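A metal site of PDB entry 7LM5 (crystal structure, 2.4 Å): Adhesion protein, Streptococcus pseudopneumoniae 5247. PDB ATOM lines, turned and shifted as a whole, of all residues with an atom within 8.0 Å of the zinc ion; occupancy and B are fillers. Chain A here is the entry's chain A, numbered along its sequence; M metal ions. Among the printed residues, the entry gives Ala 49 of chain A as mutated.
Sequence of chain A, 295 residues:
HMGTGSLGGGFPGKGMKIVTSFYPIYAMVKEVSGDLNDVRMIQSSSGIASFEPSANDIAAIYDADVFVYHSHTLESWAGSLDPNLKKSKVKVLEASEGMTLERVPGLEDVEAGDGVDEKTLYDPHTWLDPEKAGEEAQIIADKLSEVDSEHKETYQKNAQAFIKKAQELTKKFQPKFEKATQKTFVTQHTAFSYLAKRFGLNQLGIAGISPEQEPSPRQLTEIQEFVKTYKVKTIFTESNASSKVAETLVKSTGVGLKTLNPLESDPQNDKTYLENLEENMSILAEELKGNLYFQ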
ATOM      1  N   PHE A  22     -13.166 -27.870 -18.926  1.00  0.00           N
ATOM      2  CA  PHE A  22     -12.203 -27.298 -19.893  1.00  0.00           C
ATOM      3  C   PHE A  22     -11.745 -28.391 -20.864  1.00  0.00           C
ATOM      4  O   PHE A  22     -12.119 -29.526 -20.678  1.00  0.00           O
ATOM      5  CB  PHE A  22     -11.140 -26.426 -19.209  1.00  0.00           C
ATOM      6  CG  PHE A  22      -9.917 -27.120 -18.671  1.00  0.00           C
ATOM      7  CD1 PHE A  22     -10.035 -28.212 -17.845  1.00  0.00           C
ATOM      8  CD2 PHE A  22      -8.663 -26.650 -18.965  1.00  0.00           C
ATOM      9  CE1 PHE A  22      -8.911 -28.853 -17.350  1.00  0.00           C
ATOM     10  CE2 PHE A  22      -7.544 -27.287 -18.463  1.00  0.00           C
ATOM     11  CZ  PHE A  22      -7.676 -28.384 -17.669  1.00  0.00           C
ATOM     12  N   ALA A  49      -7.771 -20.225 -16.713  1.00  0.00           N
ATOM     13  CA  ALA A  49      -6.920 -19.315 -15.956  1.00  0.00           C
ATOM     14  C   ALA A  49      -7.748 -18.481 -14.980  1.00  0.00           C
ATOM     15  O   ALA A  49      -7.639 -18.644 -13.765  1.00  0.00           O
ATOM     16  CB  ALA A  49      -6.139 -18.423 -16.899  1.00  0.00           C
ATOM     17  N   PHE A  51     -11.112 -18.586 -14.967  1.00  0.00           N
ATOM     18  CA  PHE A  51     -12.183 -19.511 -14.599  1.00  0.00           C
ATOM     19  C   PHE A  51     -13.415 -18.681 -14.225  1.00  0.00           C
ATOM     20  O   PHE A  51     -13.741 -17.731 -14.961  1.00  0.00           O
ATOM     21  CB  PHE A  51     -11.687 -20.468 -13.520  1.00  0.00           C
ATOM     22  CG  PHE A  51     -10.632 -21.428 -14.011  1.00  0.00           C
ATOM     23  CD1 PHE A  51     -10.957 -22.458 -14.875  1.00  0.00           C
ATOM     24  CD2 PHE A  51      -9.319 -21.282 -13.605  1.00  0.00           C
ATOM     25  CE1 PHE A  51      -9.994 -23.332 -15.329  1.00  0.00           C
ATOM     26  CE2 PHE A  51      -8.348 -22.157 -14.053  1.00  0.00           C
ATOM     27  CZ  PHE A  51      -8.686 -23.182 -14.915  1.00  0.00           C
ATOM     28  N   LEU A  74      -7.648 -27.056  -9.288  1.00  0.00           N
ATOM     29  CA  LEU A  74      -7.751 -26.215 -10.462  1.00  0.00           C
ATOM     30  C   LEU A  74      -9.087 -25.476 -10.467  1.00  0.00           C
ATOM     31  O   LEU A  74      -9.147 -24.288 -10.159  1.00  0.00           O
ATOM     32  CB  LEU A  74      -7.595 -27.037 -11.742  1.00  0.00           C
ATOM     33  CG  LEU A  74      -7.567 -26.247 -13.051  1.00  0.00           C
ATOM     34  CD1 LEU A  74      -6.395 -25.273 -13.073  1.00  0.00           C
ATOM     35  CD2 LEU A  74      -7.512 -27.185 -14.246  1.00  0.00           C
ATOM     36  N   ASP A 123       0.490 -29.231  -7.743  1.00  0.00           N
ATOM     37  CA  ASP A 123       0.457 -28.946  -9.195  1.00  0.00           C
ATOM     38  C   ASP A 123      -0.675 -29.730  -9.841  1.00  0.00           C
ATOM     39  O   ASP A 123      -0.727 -30.901  -9.640  1.00  0.00           O
ATOM     40  CB  ASP A 123       1.804 -29.311  -9.790  1.00  0.00           C
ATOM     41  CG  ASP A 123       1.970 -28.924 -11.227  1.00  0.00           C
ATOM     42  OD1 ASP A 123       1.025 -28.489 -11.808  1.00  0.00           O
ATOM     43  OD2 ASP A 123       3.059 -29.053 -11.725  1.00  0.00           O
ATOM     44  N   PRO A 124      -1.610 -29.109 -10.593  1.00  0.00           N
ATOM     45  CA  PRO A 124      -2.686 -29.828 -11.221  1.00  0.00           C
ATOM     46  C   PRO A 124      -2.465 -30.274 -12.669  1.00  0.00           C
ATOM     47  O   PRO A 124      -3.185 -31.085 -13.099  1.00  0.00           O
ATOM     48  CB  PRO A 124      -3.761 -28.754 -11.278  1.00  0.00           C
ATOM     49  CG  PRO A 124      -2.993 -27.544 -11.581  1.00  0.00           C
ATOM     50  CD  PRO A 124      -1.730 -27.688 -10.778  1.00  0.00           C
ATOM     51  N   HIS A 125      -1.424 -29.773 -13.348  1.00  0.00           N
ATOM     52  CA  HIS A 125      -1.123 -30.030 -14.775  1.00  0.00           C
ATOM     53  C   HIS A 125      -0.653 -31.470 -15.068  1.00  0.00           C
ATOM     54  O   HIS A 125       0.386 -31.626 -15.638  1.00  0.00           O
ATOM     55  CB  HIS A 125      -0.082 -29.037 -15.278  1.00  0.00           C
ATOM     56  CG  HIS A 125      -0.418 -27.593 -15.148  1.00  0.00           C
ATOM     57  ND1 HIS A 125       0.028 -26.820 -14.132  1.00  0.00           N
ATOM     58  CD2 HIS A 125      -1.072 -26.750 -15.945  1.00  0.00           C
ATOM     59  CE1 HIS A 125      -0.396 -25.603 -14.272  1.00  0.00           C
ATOM     60  NE2 HIS A 125      -1.059 -25.518 -15.374  1.00  0.00           N
ATOM     61  N   TRP A 127      -2.520 -33.651 -16.939  1.00  0.00           N
ATOM     62  CA  TRP A 127      -3.003 -34.122 -18.232  1.00  0.00           C
ATOM     63  C   TRP A 127      -1.926 -34.084 -19.314  1.00  0.00           C
ATOM     64  O   TRP A 127      -2.094 -34.736 -20.351  1.00  0.00           O
ATOM     65  CB  TRP A 127      -4.216 -33.312 -18.665  1.00  0.00           C
ATOM     66  CG  TRP A 127      -3.953 -31.840 -18.802  1.00  0.00           C
ATOM     67  CD1 TRP A 127      -3.466 -31.196 -19.907  1.00  0.00           C
ATOM     68  CD2 TRP A 127      -4.174 -30.831 -17.810  1.00  0.00           C
ATOM     69  NE1 TRP A 127      -3.367 -29.848 -19.655  1.00  0.00           N
ATOM     70  CE2 TRP A 127      -3.795 -29.594 -18.377  1.00  0.00           C
ATOM     71  CE3 TRP A 127      -4.648 -30.857 -16.495  1.00  0.00           C
ATOM     72  CZ2 TRP A 127      -3.871 -28.402 -17.673  1.00  0.00           C
ATOM     73  CZ3 TRP A 127      -4.732 -29.664 -15.797  1.00  0.00           C
ATOM     74  CH2 TRP A 127      -4.348 -28.447 -16.390  1.00  0.00           C
ATOM     75  N   LEU A 128      -0.840 -33.339 -19.102  1.00  0.00           N
ATOM     76  CA  LEU A 128       0.229 -33.292 -20.089  1.00  0.00           C
ATOM     77  C   LEU A 128       1.195 -34.470 -19.985  1.00  0.00           C
ATOM     78  O   LEU A 128       2.065 -34.614 -20.848  1.00  0.00           O
ATOM     79  CB  LEU A 128       0.985 -31.972 -19.970  1.00  0.00           C
ATOM     80  CG  LEU A 128       0.116 -30.747 -20.283  1.00  0.00           C
ATOM     81  CD1 LEU A 128       0.905 -29.456 -20.112  1.00  0.00           C
ATOM     82  CD2 LEU A 128      -0.457 -30.849 -21.687  1.00  0.00           C
ATOM     83  N   HIS A 189       4.305 -20.420 -18.539  1.00  0.00           N
ATOM     84  CA  HIS A 189       3.959 -20.604 -17.133  1.00  0.00           C
ATOM     85  C   HIS A 189       4.223 -22.053 -16.742  1.00  0.00           C
ATOM     86  O   HIS A 189       4.475 -22.907 -17.584  1.00  0.00           O
ATOM     87  CB  HIS A 189       2.506 -20.197 -16.844  1.00  0.00           C
ATOM     88  CG  HIS A 189       1.477 -21.177 -17.302  1.00  0.00           C
ATOM     89  ND1 HIS A 189       1.163 -21.365 -18.630  1.00  0.00           N
ATOM     90  CD2 HIS A 189       0.670 -22.014 -16.604  1.00  0.00           C
ATOM     91  CE1 HIS A 189       0.226 -22.279 -18.731  1.00  0.00           C
ATOM     92  NE2 HIS A 189      -0.100 -22.692 -17.521  1.00  0.00           N
ATOM     93  N   THR A 190       4.189 -22.304 -15.432  1.00  0.00           N
ATOM     94  CA  THR A 190       4.607 -23.601 -14.872  1.00  0.00           C
ATOM     95  C   THR A 190       3.497 -24.613 -15.091  1.00  0.00           C
ATOM     96  O   THR A 190       2.661 -24.894 -14.219  1.00  0.00           O
ATOM     97  CB  THR A 190       4.958 -23.447 -13.396  1.00  0.00           C
ATOM     98  OG1 THR A 190       5.852 -22.344 -13.226  1.00  0.00           O
ATOM     99  CG2 THR A 190       5.617 -24.714 -12.873  1.00  0.00           C
ATOM    100  N   ALA A 191       3.487 -25.193 -16.296  1.00  0.00           N
ATOM    101  CA  ALA A 191       2.456 -26.140 -16.681  1.00  0.00           C
ATOM    102  C   ALA A 191       2.990 -27.483 -17.165  1.00  0.00           C
ATOM    103  O   ALA A 191       2.205 -28.421 -17.323  1.00  0.00           O
ATOM    104  CB  ALA A 191       1.566 -25.541 -17.786  1.00  0.00           C
ATOM    105  N   PHE A 192       4.287 -27.608 -17.420  1.00  0.00           N
ATOM    106  CA  PHE A 192       4.866 -28.813 -18.013  1.00  0.00           C
ATOM    107  C   PHE A 192       5.741 -29.574 -17.029  1.00  0.00           C
ATOM    108  O   PHE A 192       6.690 -30.254 -17.437  1.00  0.00           O
ATOM    109  CB  PHE A 192       5.658 -28.459 -19.271  1.00  0.00           C
ATOM    110  CG  PHE A 192       4.821 -27.790 -20.337  1.00  0.00           C
ATOM    111  CD1 PHE A 192       4.179 -28.537 -21.303  1.00  0.00           C
ATOM    112  CD2 PHE A 192       4.693 -26.407 -20.363  1.00  0.00           C
ATOM    113  CE1 PHE A 192       3.415 -27.929 -22.274  1.00  0.00           C
ATOM    114  CE2 PHE A 192       3.933 -25.790 -21.338  1.00  0.00           C
ATOM    115  CZ  PHE A 192       3.292 -26.556 -22.292  1.00  0.00           C
ATOM    116  N   GLY A 208       3.866 -18.646 -12.570  1.00  0.00           N
ATOM    117  CA  GLY A 208       3.655 -19.780 -11.693  1.00  0.00           C
ATOM    118  C   GLY A 208       2.691 -20.793 -12.261  1.00  0.00           C
ATOM    119  O   GLY A 208       2.530 -20.933 -13.484  1.00  0.00           O
ATOM    120  N   ILE A 209       2.029 -21.515 -11.353  1.00  0.00           N
ATOM    121  CA  ILE A 209       1.037 -22.515 -11.763  1.00  0.00           C
ATOM    122  C   ILE A 209      -0.054 -21.870 -12.607  1.00  0.00           C
ATOM    123  O   ILE A 209      -0.496 -22.432 -13.613  1.00  0.00           O
ATOM    124  CB  ILE A 209       0.460 -23.222 -10.528  1.00  0.00           C
ATOM    125  CG1 ILE A 209       1.512 -24.141  -9.909  1.00  0.00           C
ATOM    126  CG2 ILE A 209      -0.801 -24.004 -10.879  1.00  0.00           C
ATOM    127  CD1 ILE A 209       1.890 -25.314 -10.800  1.00  0.00           C
ATOM    128  N   SER A 210      -0.503 -20.679 -12.209  1.00  0.00           N
ATOM    129  CA  SER A 210      -1.488 -19.954 -12.997  1.00  0.00           C
ATOM    130  C   SER A 210      -0.808 -18.908 -13.866  1.00  0.00           C
ATOM    131  O   SER A 210       0.174 -18.292 -13.432  1.00  0.00           O
ATOM    132  CB  SER A 210      -2.507 -19.263 -12.088  1.00  0.00           C
ATOM    133  OG  SER A 210      -3.162 -20.208 -11.256  1.00  0.00           O
ATOM    134  N   PRO A 211      -1.292 -18.689 -15.089  1.00  0.00           N
ATOM    135  CA  PRO A 211      -0.682 -17.672 -15.950  1.00  0.00           C
ATOM    136  C   PRO A 211      -0.774 -16.267 -15.396  1.00  0.00           C
ATOM    137  O   PRO A 211       0.006 -15.399 -15.800  1.00  0.00           O
ATOM    138  CB  PRO A 211      -1.466 -17.799 -17.273  1.00  0.00           C
ATOM    139  CG  PRO A 211      -2.113 -19.154 -17.208  1.00  0.00           C
ATOM    140  CD  PRO A 211      -2.399 -19.399 -15.756  1.00  0.00           C
ATOM    141  N   GLU A 238       2.728 -19.179 -25.384  1.00  0.00           N
ATOM    142  CA  GLU A 238       1.397 -19.730 -25.588  1.00  0.00           C
ATOM    143  C   GLU A 238       0.650 -18.893 -26.617  1.00  0.00           C
ATOM    144  O   GLU A 238       0.833 -17.675 -26.700  1.00  0.00           O
ATOM    145  CB  GLU A 238       0.609 -19.783 -24.275  1.00  0.00           C
ATOM    146  CG  GLU A 238       1.056 -20.871 -23.317  1.00  0.00           C
ATOM    147  CD  GLU A 238       0.423 -20.751 -21.950  1.00  0.00           C
ATOM    148  OE1 GLU A 238       1.145 -20.426 -20.986  1.00  0.00           O
ATOM    149  OE2 GLU A 238      -0.805 -20.967 -21.840  1.00  0.00           O
ATOM    150  N   PRO A 262      -0.086 -25.794 -23.670  1.00  0.00           N
ATOM    151  CA  PRO A 262      -0.403 -26.686 -22.544  1.00  0.00           C
ATOM    152  C   PRO A 262      -1.783 -27.326 -22.628  1.00  0.00           C
ATOM    153  O   PRO A 262      -2.181 -28.005 -21.682  1.00  0.00           O
ATOM    154  CB  PRO A 262      -0.311 -25.746 -21.328  1.00  0.00           C
ATOM    155  CG  PRO A 262      -0.657 -24.404 -21.876  1.00  0.00           C
ATOM    156  CD  PRO A 262      -0.109 -24.373 -23.275  1.00  0.00           C
ATOM    157  N   GLU A 264      -4.733 -26.038 -22.410  1.00  0.00           N
ATOM    158  CA  GLU A 264      -5.707 -25.505 -21.467  1.00  0.00           C
ATOM    159  C   GLU A 264      -6.879 -24.844 -22.164  1.00  0.00           C
ATOM    160  O   GLU A 264      -7.933 -24.643 -21.534  1.00  0.00           O
ATOM    161  CB  GLU A 264      -5.041 -24.507 -20.513  1.00  0.00           C
ATOM    162  CG  GLU A 264      -4.002 -25.163 -19.618  1.00  0.00           C
ATOM    163  CD  GLU A 264      -3.388 -24.199 -18.616  1.00  0.00           C
ATOM    164  OE1 GLU A 264      -3.797 -23.015 -18.595  1.00  0.00           O
ATOM    165  OE2 GLU A 264      -2.500 -24.625 -17.853  1.00  0.00           O
HETATM  166 ZN    ZN M   1      -1.803 -23.928 -16.191  1.00  0.00          ZN
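ND1 of His 125 sits close to O of Thr 190 (3.3 Å). The side-chain carboxylate of Glu 238 is in hydrogen-bond range of a ring nitrogen (ND1) of His 189 (2.5 Å). A ring nitrogen (ND1) of His 125 lies within hydrogen-bond range of the side-chain carboxylate of Asp 123 (3.0 Å).
The side-chain carboxylate (OE2) of Glu 264 binds the zinc ion (1.9 Å). NE2 of His 125 is bound to the zinc ion, 1.9 Å away. A ring nitrogen (NE2) of His 189 is bound to the zinc ion, at 2.5 Å.
Ile 209 touches the zinc ion (O to ZN, 3.3 Å). Four residues have an atom within 4 Å of the zinc ion: His 125, His 189, Ile 209 and Glu 264. The nearest printed residue that does not touch the zinc ion is Ala 191 (4.1 Å).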
